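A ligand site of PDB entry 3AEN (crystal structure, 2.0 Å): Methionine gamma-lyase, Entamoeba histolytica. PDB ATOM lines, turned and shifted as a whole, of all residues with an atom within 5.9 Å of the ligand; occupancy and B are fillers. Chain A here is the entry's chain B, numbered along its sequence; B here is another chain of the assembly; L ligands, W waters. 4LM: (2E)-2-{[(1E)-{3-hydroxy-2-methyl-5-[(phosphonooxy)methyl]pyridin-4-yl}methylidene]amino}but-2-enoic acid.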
ATOM      1  N   SER A  82       2.969  20.244 -16.095  1.00  0.00           N
ATOM      2  CA  SER A  82       3.641  21.252 -15.261  1.00  0.00           C
ATOM      3  C   SER A  82       4.803  20.597 -14.568  1.00  0.00           C
ATOM      4  O   SER A  82       4.869  19.356 -14.491  1.00  0.00           O
ATOM      5  CB  SER A  82       2.697  21.878 -14.214  1.00  0.00           C
ATOM      6  OG  SER A  82       2.152  20.890 -13.337  1.00  0.00           O
ATOM      7  N   GLY A  83       5.746  21.415 -14.103  1.00  0.00           N
ATOM      8  CA  GLY A  83       6.783  20.973 -13.198  1.00  0.00           C
ATOM      9  C   GLY A  83       6.218  20.264 -11.980  1.00  0.00           C
ATOM     10  O   GLY A  83       6.763  19.242 -11.557  1.00  0.00           O
ATOM     11  N   MET A  84       5.115  20.767 -11.407  1.00  0.00           N
ATOM     12  CA  MET A  84       4.557  20.096 -10.239  1.00  0.00           C
ATOM     13  C   MET A  84       4.035  18.686 -10.589  1.00  0.00           C
ATOM     14  O   MET A  84       4.098  17.772  -9.756  1.00  0.00           O
ATOM     15  CB  MET A  84       3.464  20.937  -9.558  1.00  0.00           C
ATOM     16  CG  MET A  84       3.986  22.234  -8.846  1.00  0.00           C
ATOM     17  SD  MET A  84       5.525  22.002  -7.892  1.00  0.00           S
ATOM     18  CE  MET A  84       4.948  20.755  -6.700  1.00  0.00           C
ATOM     19  N   GLY A  85       3.512  18.513 -11.813  1.00  0.00           N
ATOM     20  CA  GLY A  85       3.153  17.190 -12.330  1.00  0.00           C
ATOM     21  C   GLY A  85       4.373  16.262 -12.448  1.00  0.00           C
ATOM     22  O   GLY A  85       4.314  15.074 -12.094  1.00  0.00           O
ATOM     23  N   ILE A  87       7.118  16.517 -10.602  1.00  0.00           N
ATOM     24  CA  ILE A  87       7.571  16.277  -9.228  1.00  0.00           C
ATOM     25  C   ILE A  87       6.652  15.277  -8.501  1.00  0.00           C
ATOM     26  O   ILE A  87       7.126  14.335  -7.876  1.00  0.00           O
ATOM     27  CB  ILE A  87       7.699  17.616  -8.408  1.00  0.00           C
ATOM     28  CG1 ILE A  87       8.798  18.491  -8.992  1.00  0.00           C
ATOM     29  CG2 ILE A  87       7.923  17.331  -6.918  1.00  0.00           C
ATOM     30  CD1 ILE A  87       8.796  19.952  -8.503  1.00  0.00           C
ATOM     31  N   TYR A 108      11.372  25.061  -3.933  1.00  0.00           N
ATOM     32  CA  TYR A 108      10.262  25.787  -4.497  1.00  0.00           C
ATOM     33  C   TYR A 108       9.019  25.655  -3.575  1.00  0.00           C
ATOM     34  O   TYR A 108       8.745  24.583  -3.022  1.00  0.00           O
ATOM     35  CB  TYR A 108      10.008  25.327  -5.953  1.00  0.00           C
ATOM     36  CG  TYR A 108       8.735  25.911  -6.515  1.00  0.00           C
ATOM     37  CD1 TYR A 108       8.562  27.292  -6.581  1.00  0.00           C
ATOM     38  CD2 TYR A 108       7.682  25.094  -6.909  1.00  0.00           C
ATOM     39  CE1 TYR A 108       7.376  27.851  -7.022  1.00  0.00           C
ATOM     40  CE2 TYR A 108       6.501  25.640  -7.375  1.00  0.00           C
ATOM     41  CZ  TYR A 108       6.347  27.023  -7.430  1.00  0.00           C
ATOM     42  OH  TYR A 108       5.176  27.611  -7.882  1.00  0.00           O
ATOM     43  N   THR A 111       6.534  22.707  -4.027  1.00  0.00           N
ATOM     44  CA  THR A 111       7.194  21.472  -3.617  1.00  0.00           C
ATOM     45  C   THR A 111       7.084  21.306  -2.076  1.00  0.00           C
ATOM     46  O   THR A 111       6.725  20.232  -1.589  1.00  0.00           O
ATOM     47  CB  THR A 111       8.644  21.419  -4.110  1.00  0.00           C
ATOM     48  OG1 THR A 111       8.694  21.732  -5.521  1.00  0.00           O
ATOM     49  CG2 THR A 111       9.238  20.022  -3.869  1.00  0.00           C
ATOM     50  N   TYR A 149      15.284  13.719  -2.049  1.00  0.00           N
ATOM     51  CA  TYR A 149      14.853  14.658  -3.073  1.00  0.00           C
ATOM     52  C   TYR A 149      15.622  15.973  -2.895  1.00  0.00           C
ATOM     53  O   TYR A 149      15.650  16.537  -1.800  1.00  0.00           O
ATOM     54  CB  TYR A 149      13.327  14.869  -3.015  1.00  0.00           C
ATOM     55  CG  TYR A 149      12.799  15.832  -4.065  1.00  0.00           C
ATOM     56  CD1 TYR A 149      12.913  17.211  -3.904  1.00  0.00           C
ATOM     57  CD2 TYR A 149      12.200  15.350  -5.233  1.00  0.00           C
ATOM     58  CE1 TYR A 149      12.424  18.104  -4.871  1.00  0.00           C
ATOM     59  CE2 TYR A 149      11.714  16.234  -6.202  1.00  0.00           C
ATOM     60  CZ  TYR A 149      11.830  17.591  -6.006  1.00  0.00           C
ATOM     61  OH  TYR A 149      11.355  18.459  -6.949  1.00  0.00           O
ATOM     62  N   GLU A 151      17.006  19.910  -4.707  1.00  0.00           N
ATOM     63  CA  GLU A 151      17.136  20.993  -5.701  1.00  0.00           C
ATOM     64  C   GLU A 151      18.501  21.620  -5.465  1.00  0.00           C
ATOM     65  O   GLU A 151      18.827  21.958  -4.319  1.00  0.00           O
ATOM     66  CB  GLU A 151      16.135  22.117  -5.463  1.00  0.00           C
ATOM     67  CG  GLU A 151      14.735  21.920  -5.962  1.00  0.00           C
ATOM     68  CD  GLU A 151      13.872  23.118  -5.634  1.00  0.00           C
ATOM     69  OE1 GLU A 151      14.395  24.257  -5.665  1.00  0.00           O
ATOM     70  OE2 GLU A 151      12.672  22.916  -5.352  1.00  0.00           O
ATOM     71  N   ASN A 155      15.957  26.833  -5.009  1.00  0.00           N
ATOM     72  CA  ASN A 155      15.080  27.983  -5.232  1.00  0.00           C
ATOM     73  C   ASN A 155      14.567  28.490  -3.876  1.00  0.00           C
ATOM     74  O   ASN A 155      13.826  27.759  -3.194  1.00  0.00           O
ATOM     75  CB  ASN A 155      13.926  27.598  -6.163  1.00  0.00           C
ATOM     76  CG  ASN A 155      12.956  28.773  -6.443  1.00  0.00           C
ATOM     77  OD1 ASN A 155      13.060  29.848  -5.876  1.00  0.00           O
ATOM     78  ND2 ASN A 155      11.999  28.541  -7.341  1.00  0.00           N
ATOM     79  N   ASP A 180      15.794  17.942  -8.835  1.00  0.00           N
ATOM     80  CA  ASP A 180      15.131  18.991  -9.588  1.00  0.00           C
ATOM     81  C   ASP A 180      16.190  19.966 -10.109  1.00  0.00           C
ATOM     82  O   ASP A 180      16.809  20.708  -9.341  1.00  0.00           O
ATOM     83  CB  ASP A 180      14.126  19.725  -8.697  1.00  0.00           C
ATOM     84  CG  ASP A 180      13.357  20.791  -9.458  1.00  0.00           C
ATOM     85  OD1 ASP A 180      13.825  21.208 -10.552  1.00  0.00           O
ATOM     86  OD2 ASP A 180      12.277  21.203  -8.988  1.00  0.00           O
ATOM     87  N   THR A 182      15.759  22.330 -12.473  1.00  0.00           N
ATOM     88  CA  THR A 182      15.102  23.473 -13.102  1.00  0.00           C
ATOM     89  C   THR A 182      16.012  24.706 -13.198  1.00  0.00           C
ATOM     90  O   THR A 182      16.137  25.292 -14.267  1.00  0.00           O
ATOM     91  CB  THR A 182      13.825  23.884 -12.321  1.00  0.00           C
ATOM     92  OG1 THR A 182      12.882  22.807 -12.376  1.00  0.00           O
ATOM     93  CG2 THR A 182      13.191  25.134 -12.926  1.00  0.00           C
ATOM     94  N   PHE A 183      16.679  25.066 -12.098  1.00  0.00           N
ATOM     95  CA  PHE A 183      17.429  26.332 -12.020  1.00  0.00           C
ATOM     96  C   PHE A 183      18.615  26.411 -12.961  1.00  0.00           C
ATOM     97  O   PHE A 183      19.048  27.507 -13.314  1.00  0.00           O
ATOM     98  CB  PHE A 183      17.869  26.631 -10.579  1.00  0.00           C
ATOM     99  CG  PHE A 183      17.018  27.666  -9.893  1.00  0.00           C
ATOM    100  CD1 PHE A 183      15.633  27.654 -10.070  1.00  0.00           C
ATOM    101  CD2 PHE A 183      17.589  28.632  -9.085  1.00  0.00           C
ATOM    102  CE1 PHE A 183      14.821  28.596  -9.433  1.00  0.00           C
ATOM    103  CE2 PHE A 183      16.781  29.595  -8.441  1.00  0.00           C
ATOM    104  CZ  PHE A 183      15.408  29.580  -8.630  1.00  0.00           C
ATOM    105  N   LEU A 200      14.639  15.979 -13.138  1.00  0.00           N
ATOM    106  CA  LEU A 200      13.373  16.564 -13.562  1.00  0.00           C
ATOM    107  C   LEU A 200      13.484  18.071 -13.675  1.00  0.00           C
ATOM    108  O   LEU A 200      14.345  18.683 -13.037  1.00  0.00           O
ATOM    109  CB  LEU A 200      12.237  16.150 -12.611  1.00  0.00           C
ATOM    110  CG  LEU A 200      12.265  16.646 -11.160  1.00  0.00           C
ATOM    111  CD1 LEU A 200      11.680  18.037 -11.066  1.00  0.00           C
ATOM    112  CD2 LEU A 200      11.459  15.683 -10.313  1.00  0.00           C
ATOM    113  N   HIS A 201      12.609  18.662 -14.497  1.00  0.00           N
ATOM    114  CA  HIS A 201      12.596  20.099 -14.741  1.00  0.00           C
ATOM    115  C   HIS A 201      11.187  20.575 -14.836  1.00  0.00           C
ATOM    116  O   HIS A 201      10.297  19.865 -15.360  1.00  0.00           O
ATOM    117  CB  HIS A 201      13.284  20.435 -16.075  1.00  0.00           C
ATOM    118  CG  HIS A 201      14.695  19.975 -16.133  1.00  0.00           C
ATOM    119  ND1 HIS A 201      15.758  20.788 -15.823  1.00  0.00           N
ATOM    120  CD2 HIS A 201      15.226  18.751 -16.394  1.00  0.00           C
ATOM    121  CE1 HIS A 201      16.877  20.094 -15.910  1.00  0.00           C
ATOM    122  NE2 HIS A 201      16.581  18.862 -16.249  1.00  0.00           N
ATOM    123  N   SER A 202      10.984  21.790 -14.327  1.00  0.00           N
ATOM    124  CA  SER A 202       9.883  22.612 -14.807  1.00  0.00           C
ATOM    125  C   SER A 202      10.323  23.104 -16.203  1.00  0.00           C
ATOM    126  O   SER A 202      11.272  23.894 -16.335  1.00  0.00           O
ATOM    127  CB  SER A 202       9.642  23.806 -13.886  1.00  0.00           C
ATOM    128  OG  SER A 202       8.637  24.646 -14.442  1.00  0.00           O
ATOM    129  N   VAL A 203       9.664  22.595 -17.234  1.00  0.00           N
ATOM    130  CA  VAL A 203       9.948  22.995 -18.611  1.00  0.00           C
ATOM    131  C   VAL A 203       9.512  24.459 -18.826  1.00  0.00           C
ATOM    132  O   VAL A 203      10.043  25.161 -19.701  1.00  0.00           O
ATOM    133  CB  VAL A 203       9.305  22.023 -19.601  1.00  0.00           C
ATOM    134  CG1 VAL A 203       9.376  22.553 -21.026  1.00  0.00           C
ATOM    135  CG2 VAL A 203      10.013  20.683 -19.507  1.00  0.00           C
ATOM    136  N   SER A 204       8.608  24.917 -17.969  1.00  0.00           N
ATOM    137  CA  SER A 204       8.088  26.286 -17.954  1.00  0.00           C
ATOM    138  C   SER A 204       9.197  27.327 -17.917  1.00  0.00           C
ATOM    139  O   SER A 204       8.998  28.461 -18.358  1.00  0.00           O
ATOM    140  CB  SER A 204       7.203  26.451 -16.696  1.00  0.00           C
ATOM    141  OG  SER A 204       6.317  25.342 -16.528  1.00  0.00           O
ATOM    142  N   LYS A 205      10.350  26.943 -17.369  1.00  0.00           N
ATOM    143  CA  LYS A 205      11.463  27.871 -17.210  1.00  0.00           C
ATOM    144  C   LYS A 205      12.414  27.838 -18.414  1.00  0.00           C
ATOM    145  O   LYS A 205      12.000  28.110 -19.546  1.00  0.00           O
ATOM    146  CB  LYS A 205      12.203  27.615 -15.876  1.00  0.00           C
ATOM    147  CG  LYS A 205      11.285  27.380 -14.652  1.00  0.00           C
ATOM    148  CD  LYS A 205      10.102  28.344 -14.585  1.00  0.00           C
ATOM    149  CE  LYS A 205       9.401  28.233 -13.253  1.00  0.00           C
ATOM    150  NZ  LYS A 205       8.010  28.783 -13.397  1.00  0.00           N
ATOM    151  N   ILE A 214       3.500  26.216 -19.621  1.00  0.00           N
ATOM    152  CA  ILE A 214       3.752  25.492 -18.365  1.00  0.00           C
ATOM    153  C   ILE A 214       3.876  24.019 -18.707  1.00  0.00           C
ATOM    154  O   ILE A 214       2.994  23.457 -19.351  1.00  0.00           O
ATOM    155  CB  ILE A 214       2.552  25.622 -17.379  1.00  0.00           C
ATOM    156  CG1 ILE A 214       2.101  27.079 -17.240  1.00  0.00           C
ATOM    157  CG2 ILE A 214       2.828  24.884 -16.022  1.00  0.00           C
ATOM    158  CD1 ILE A 214       2.828  27.880 -16.250  1.00  0.00           C
ATOM    159  N   GLY A 215       4.969  23.388 -18.292  1.00  0.00           N
ATOM    160  CA  GLY A 215       5.182  21.972 -18.529  1.00  0.00           C
ATOM    161  C   GLY A 215       6.240  21.429 -17.593  1.00  0.00           C
ATOM    162  O   GLY A 215       7.017  22.195 -17.002  1.00  0.00           O
ATOM    163  N   GLY A 216       6.278  20.111 -17.467  1.00  0.00           N
ATOM    164  CA  GLY A 216       7.258  19.435 -16.660  1.00  0.00           C
ATOM    165  C   GLY A 216       7.826  18.296 -17.471  1.00  0.00           C
ATOM    166  O   GLY A 216       7.207  17.808 -18.432  1.00  0.00           O
ATOM    167  N   VAL A 331       6.467  36.624 -11.004  1.00  0.00           N
ATOM    168  CA  VAL A 331       7.039  35.337 -10.612  1.00  0.00           C
ATOM    169  C   VAL A 331       7.417  34.536 -11.877  1.00  0.00           C
ATOM    170  O   VAL A 331       7.126  34.979 -12.993  1.00  0.00           O
ATOM    171  CB  VAL A 331       6.122  34.523  -9.647  1.00  0.00           C
ATOM    172  CG1 VAL A 331       5.778  35.354  -8.382  1.00  0.00           C
ATOM    173  CG2 VAL A 331       4.865  33.997 -10.353  1.00  0.00           C
ATOM    174  N   SER A 332       8.095  33.404 -11.676  1.00  0.00           N
ATOM    175  CA  SER A 332       8.656  32.565 -12.727  1.00  0.00           C
ATOM    176  C   SER A 332      10.107  32.940 -13.031  1.00  0.00           C
ATOM    177  O   SER A 332      10.655  33.888 -12.461  1.00  0.00           O
ATOM    178  CB  SER A 332       7.809  32.560 -14.012  1.00  0.00           C
ATOM    179  OG  SER A 332       8.193  31.464 -14.846  1.00  0.00           O
ATOM    180  N   LEU A 333      10.734  32.187 -13.917  1.00  0.00           N
ATOM    181  CA  LEU A 333      12.120  32.407 -14.230  1.00  0.00           C
ATOM    182  C   LEU A 333      12.496  31.712 -15.524  1.00  0.00           C
ATOM    183  O   LEU A 333      11.714  30.962 -16.100  1.00  0.00           O
ATOM    184  CB  LEU A 333      13.017  31.886 -13.091  1.00  0.00           C
ATOM    185  CG  LEU A 333      12.962  30.381 -12.829  1.00  0.00           C
ATOM    186  CD1 LEU A 333      14.363  29.770 -12.934  1.00  0.00           C
ATOM    187  CD2 LEU A 333      12.359  30.181 -11.438  1.00  0.00           C
ATOM    188  N   GLU A 341      11.370  39.492  -8.549  1.00  0.00           N
ATOM    189  CA  GLU A 341      10.384  38.913  -7.668  1.00  0.00           C
ATOM    190  C   GLU A 341      10.760  39.122  -6.205  1.00  0.00           C
ATOM    191  O   GLU A 341      11.942  39.268  -5.875  1.00  0.00           O
ATOM    192  CB  GLU A 341      10.367  37.419  -7.999  1.00  0.00           C
ATOM    193  CG  GLU A 341       9.248  36.670  -7.523  1.00  0.00           C
ATOM    194  CD  GLU A 341       9.585  35.798  -6.344  1.00  0.00           C
ATOM    195  OE1 GLU A 341      10.595  35.048  -6.347  1.00  0.00           O
ATOM    196  OE2 GLU A 341       8.793  35.852  -5.413  1.00  0.00           O
ATOM    197  N   THR A 347       6.642  33.938  -4.233  1.00  0.00           N
ATOM    198  CA  THR A 347       6.873  32.508  -4.517  1.00  0.00           C
ATOM    199  C   THR A 347       6.896  31.628  -3.275  1.00  0.00           C
ATOM    200  O   THR A 347       6.480  30.469  -3.331  1.00  0.00           O
ATOM    201  CB  THR A 347       8.168  32.253  -5.331  1.00  0.00           C
ATOM    202  OG1 THR A 347       9.267  32.908  -4.693  1.00  0.00           O
ATOM    203  CG2 THR A 347       8.023  32.713  -6.794  1.00  0.00           C
ATOM    204  N   HIS A 348       7.367  32.189  -2.159  1.00  0.00           N
ATOM    205  CA  HIS A 348       7.513  31.436  -0.904  1.00  0.00           C
ATOM    206  C   HIS A 348       6.693  32.029   0.219  1.00  0.00           C
ATOM    207  O   HIS A 348       7.098  31.951   1.381  1.00  0.00           O
ATOM    208  CB  HIS A 348       8.991  31.350  -0.504  1.00  0.00           C
ATOM    209  CG  HIS A 348       9.809  30.508  -1.424  1.00  0.00           C
ATOM    210  ND1 HIS A 348      10.101  30.886  -2.723  1.00  0.00           N
ATOM    211  CD2 HIS A 348      10.350  29.276  -1.268  1.00  0.00           C
ATOM    212  CE1 HIS A 348      10.807  29.933  -3.314  1.00  0.00           C
ATOM    213  NE2 HIS A 348      10.967  28.948  -2.449  1.00  0.00           N
ATOM    214  N   ARG A 367      14.740  38.315  -5.696  1.00  0.00           N
ATOM    215  CA  ARG A 367      15.219  37.303  -6.647  1.00  0.00           C
ATOM    216  C   ARG A 367      15.111  37.849  -8.072  1.00  0.00           C
ATOM    217  O   ARG A 367      14.044  38.297  -8.503  1.00  0.00           O
ATOM    218  CB  ARG A 367      14.449  35.984  -6.502  1.00  0.00           C
ATOM    219  CG  ARG A 367      15.140  34.763  -7.115  1.00  0.00           C
ATOM    220  CD  ARG A 367      14.196  33.575  -7.300  1.00  0.00           C
ATOM    221  NE  ARG A 367      13.143  33.825  -8.298  1.00  0.00           N
ATOM    222  CZ  ARG A 367      12.079  33.050  -8.490  1.00  0.00           C
ATOM    223  NH1 ARG A 367      11.904  31.935  -7.780  1.00  0.00           N
ATOM    224  NH2 ARG A 367      11.174  33.380  -9.407  1.00  0.00           N
ATOM    225  N   TYR B  53      -0.082  33.381 -12.362  1.00  0.00           N
ATOM    226  CA  TYR B  53       0.689  32.306 -12.990  1.00  0.00           C
ATOM    227  C   TYR B  53      -0.302  31.243 -13.409  1.00  0.00           C
ATOM    228  O   TYR B  53      -1.191  30.905 -12.626  1.00  0.00           O
ATOM    229  CB  TYR B  53       1.707  31.726 -11.972  1.00  0.00           C
ATOM    230  CG  TYR B  53       2.677  30.697 -12.538  1.00  0.00           C
ATOM    231  CD1 TYR B  53       3.754  31.085 -13.352  1.00  0.00           C
ATOM    232  CD2 TYR B  53       2.560  29.341 -12.219  1.00  0.00           C
ATOM    233  CE1 TYR B  53       4.684  30.116 -13.868  1.00  0.00           C
ATOM    234  CE2 TYR B  53       3.477  28.373 -12.714  1.00  0.00           C
ATOM    235  CZ  TYR B  53       4.532  28.768 -13.536  1.00  0.00           C
ATOM    236  OH  TYR B  53       5.443  27.831 -14.033  1.00  0.00           O
ATOM    237  N   ARG B  55      -0.611  28.041 -13.800  1.00  0.00           N
ATOM    238  CA  ARG B  55      -0.944  26.867 -12.935  1.00  0.00           C
ATOM    239  C   ARG B  55      -2.006  27.202 -11.858  1.00  0.00           C
ATOM    240  O   ARG B  55      -2.859  26.347 -11.503  1.00  0.00           O
ATOM    241  CB  ARG B  55       0.309  26.236 -12.274  1.00  0.00           C
ATOM    242  CG  ARG B  55      -0.048  25.114 -11.288  1.00  0.00           C
ATOM    243  CD  ARG B  55       1.116  24.092 -11.048  1.00  0.00           C
ATOM    244  NE  ARG B  55       2.390  24.786 -10.897  1.00  0.00           N
ATOM    245  CZ  ARG B  55       2.785  25.470  -9.828  1.00  0.00           C
ATOM    246  NH1 ARG B  55       2.026  25.524  -8.728  1.00  0.00           N
ATOM    247  NH2 ARG B  55       3.977  26.065  -9.847  1.00  0.00           N
ATOM    248  N   LYS B 234      -2.984  22.501  -7.801  1.00  0.00           N
ATOM    249  CA  LYS B 234      -1.799  23.359  -7.768  1.00  0.00           C
ATOM    250  C   LYS B 234      -0.505  22.564  -7.515  1.00  0.00           C
ATOM    251  O   LYS B 234       0.579  22.893  -8.064  1.00  0.00           O
ATOM    252  CB  LYS B 234      -2.022  24.458  -6.698  1.00  0.00           C
ATOM    253  CG  LYS B 234      -0.777  25.161  -6.188  1.00  0.00           C
ATOM    254  CD  LYS B 234      -1.086  26.211  -5.072  1.00  0.00           C
ATOM    255  CE  LYS B 234      -1.133  25.586  -3.667  1.00  0.00           C
ATOM    256  NZ  LYS B 234       0.186  24.978  -3.196  1.00  0.00           N
HETATM  257  C   4LM L   1       9.033  30.430  -9.378  1.00  0.00           C
HETATM  258  N   4LM L   1       8.978  28.057  -9.876  1.00  0.00           N
HETATM  259  O1  4LM L   1       9.864  30.226  -8.444  1.00  0.00           O
HETATM  260  P   4LM L   1       5.736  24.468 -12.685  1.00  0.00           P
HETATM  261  N1  4LM L   1      10.829  23.412  -9.569  1.00  0.00           N
HETATM  262  C2  4LM L   1      11.456  24.604  -9.434  1.00  0.00           C
HETATM  263  C3  4LM L   1      10.713  25.763  -9.671  1.00  0.00           C
HETATM  264  O3  4LM L   1      11.314  26.984  -9.548  1.00  0.00           O
HETATM  265  C4  4LM L   1       9.369  25.683 -10.079  1.00  0.00           C
HETATM  266  C5  4LM L   1       8.762  24.423 -10.151  1.00  0.00           C
HETATM  267  C6  4LM L   1       9.538  23.292  -9.904  1.00  0.00           C
HETATM  268  CA  4LM L   1       8.312  29.243  -9.923  1.00  0.00           C
HETATM  269  CB  4LM L   1       7.027  29.244 -10.398  1.00  0.00           C
HETATM  270  CG  4LM L   1       6.086  30.419 -10.552  1.00  0.00           C
HETATM  271  C2A 4LM L   1      12.923  24.658  -9.041  1.00  0.00           C
HETATM  272  C4A 4LM L   1       8.551  26.913 -10.263  1.00  0.00           C
HETATM  273  C5A 4LM L   1       7.305  24.241 -10.542  1.00  0.00           C
HETATM  274  OP1 4LM L   1       6.046  24.374 -14.156  1.00  0.00           O
HETATM  275  OP2 4LM L   1       5.463  25.860 -12.216  1.00  0.00           O
HETATM  276  OP3 4LM L   1       4.749  23.482 -12.134  1.00  0.00           O
HETATM  277  OP4 4LM L   1       7.166  24.112 -11.984  1.00  0.00           O
HETATM  278  O2  4LM L   1       8.807  31.578  -9.783  1.00  0.00           O
HETATM  279  O   HOH W   1      16.135  25.028  -7.777  1.00  0.00           O
HETATM  280  O   HOH W   2       4.923  30.861  -7.374  1.00  0.00           O
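The guanidinium group (NH2) of Arg 367 lies within hydrogen-bond range of the backbone carbonyl oxygen (O) of Ser 332, 3.1 Å away. The side-chain hydroxyl (OG1) of Thr 347 sits at hydrogen-bond distance from a ring nitrogen (ND1) of His 348 (2.9 Å). The backbone NH (N) of Tyr 108 sits at hydrogen-bond distance from the side-chain carboxylate (OE2) of Glu 151, 2.9 Å away. The side-chain hydroxyl of Ser 204 is in hydrogen-bond range of the backbone NH of Gly 215, 3.0 Å away. The side-chain carboxylate (OE1) of Glu 341 sits at hydrogen-bond distance from the side-chain hydroxyl (OG1) of Thr 347 (3.0 Å). The backbone carbonyl oxygen (O) of Lys 234 of chain B lies within hydrogen-bond range of the guanidinium group (NH1) of Arg 55 of chain B. N of Asn 155 is in hydrogen-bond range of OE1 of Glu 151 (3.1 Å). The side-chain hydroxyl of Ser 202 sits at hydrogen-bond distance from the side-chain hydroxyl of Ser 204.
Water W1 bridges OE1 of Glu 151 (2.8 Å) and N of Asn 155 (3.3 Å).
OG of Ser 204 lies within hydrogen-bond range of OP1 of the ligand. OP1 of the ligand is in hydrogen-bond range of N of Gly 83 (3.0 Å). An oxygen (O2) of the ligand sits at hydrogen-bond distance from the backbone NH (N) of Ser 332 (2.7 Å). OP3 of the ligand is in hydrogen-bond range of N of Met 84 (2.8 Å). An oxygen (O1) of the ligand lies within salt-bridge range of the guanidinium group of Arg 367 (2.7 Å). The side-chain carboxylate of Asp 180 lies within hydrogen-bond range of a nitrogen (N1) of the ligand (2.7 Å). The guanidinium group (NH2) of Arg 55 of chain B is in salt-bridge range of an oxygen (OP2) of the ligand (2.8 Å). O3 of the ligand is in hydrogen-bond range of ND2 of Asn 155 (2.8 Å). An oxygen (OP2) of the ligand sits at hydrogen-bond distance from the side-chain hydroxyl (OH) of Tyr 53 of chain B, at 2.7 Å. OG of Ser 202 is in hydrogen-bond range of OP1 of the ligand (2.6 Å).
Ser 82 touches the ligand (CB to OP3, 3.3 Å). CD1 of Ile 87 touches C6 of the ligand, at 3.7 Å. Tyr 108 touches the ligand. Glu 151 touches the ligand. Thr 182 touches the ligand (CB to C2A, 3.5 Å). Phe 183 touches the ligand (CE1 to O3, 3.9 Å). Lys 205 touches the ligand (NZ to CB, 3.2 Å). CG2 of Ile 214 touches OP1 of the ligand, 3.8 Å away. Gly 215 touches the ligand (O to OP1, 3.7 Å). CG2 of Val 331 touches CG of the ligand, at 3.8 Å. CD2 of Leu 333 touches O3 of the ligand, 3.9 Å away. Thr 347 touches the ligand. Hydrophobic or aromatic side chains that line the ligand: Met 84, Ile 87, Tyr 108, Phe 183, Ile 214, Val 331, Leu 333 and Tyr 53 of chain B. Within 4 Å of the ligand: Ser 82, Gly 83, Met 84, Ile 87, Tyr 108, Glu 151, Asn 155, Asp 180, Thr 182, Phe 183, Ser 202, Ser 204, Lys 205, Ile 214, Gly 215, Val 331, Ser 332, Leu 333, Thr 347, Arg 367, Tyr 53 of chain B and Arg 55 of chain B. The nearest printed residue that does not touch the ligand is Thr 111 (4.7 Å).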
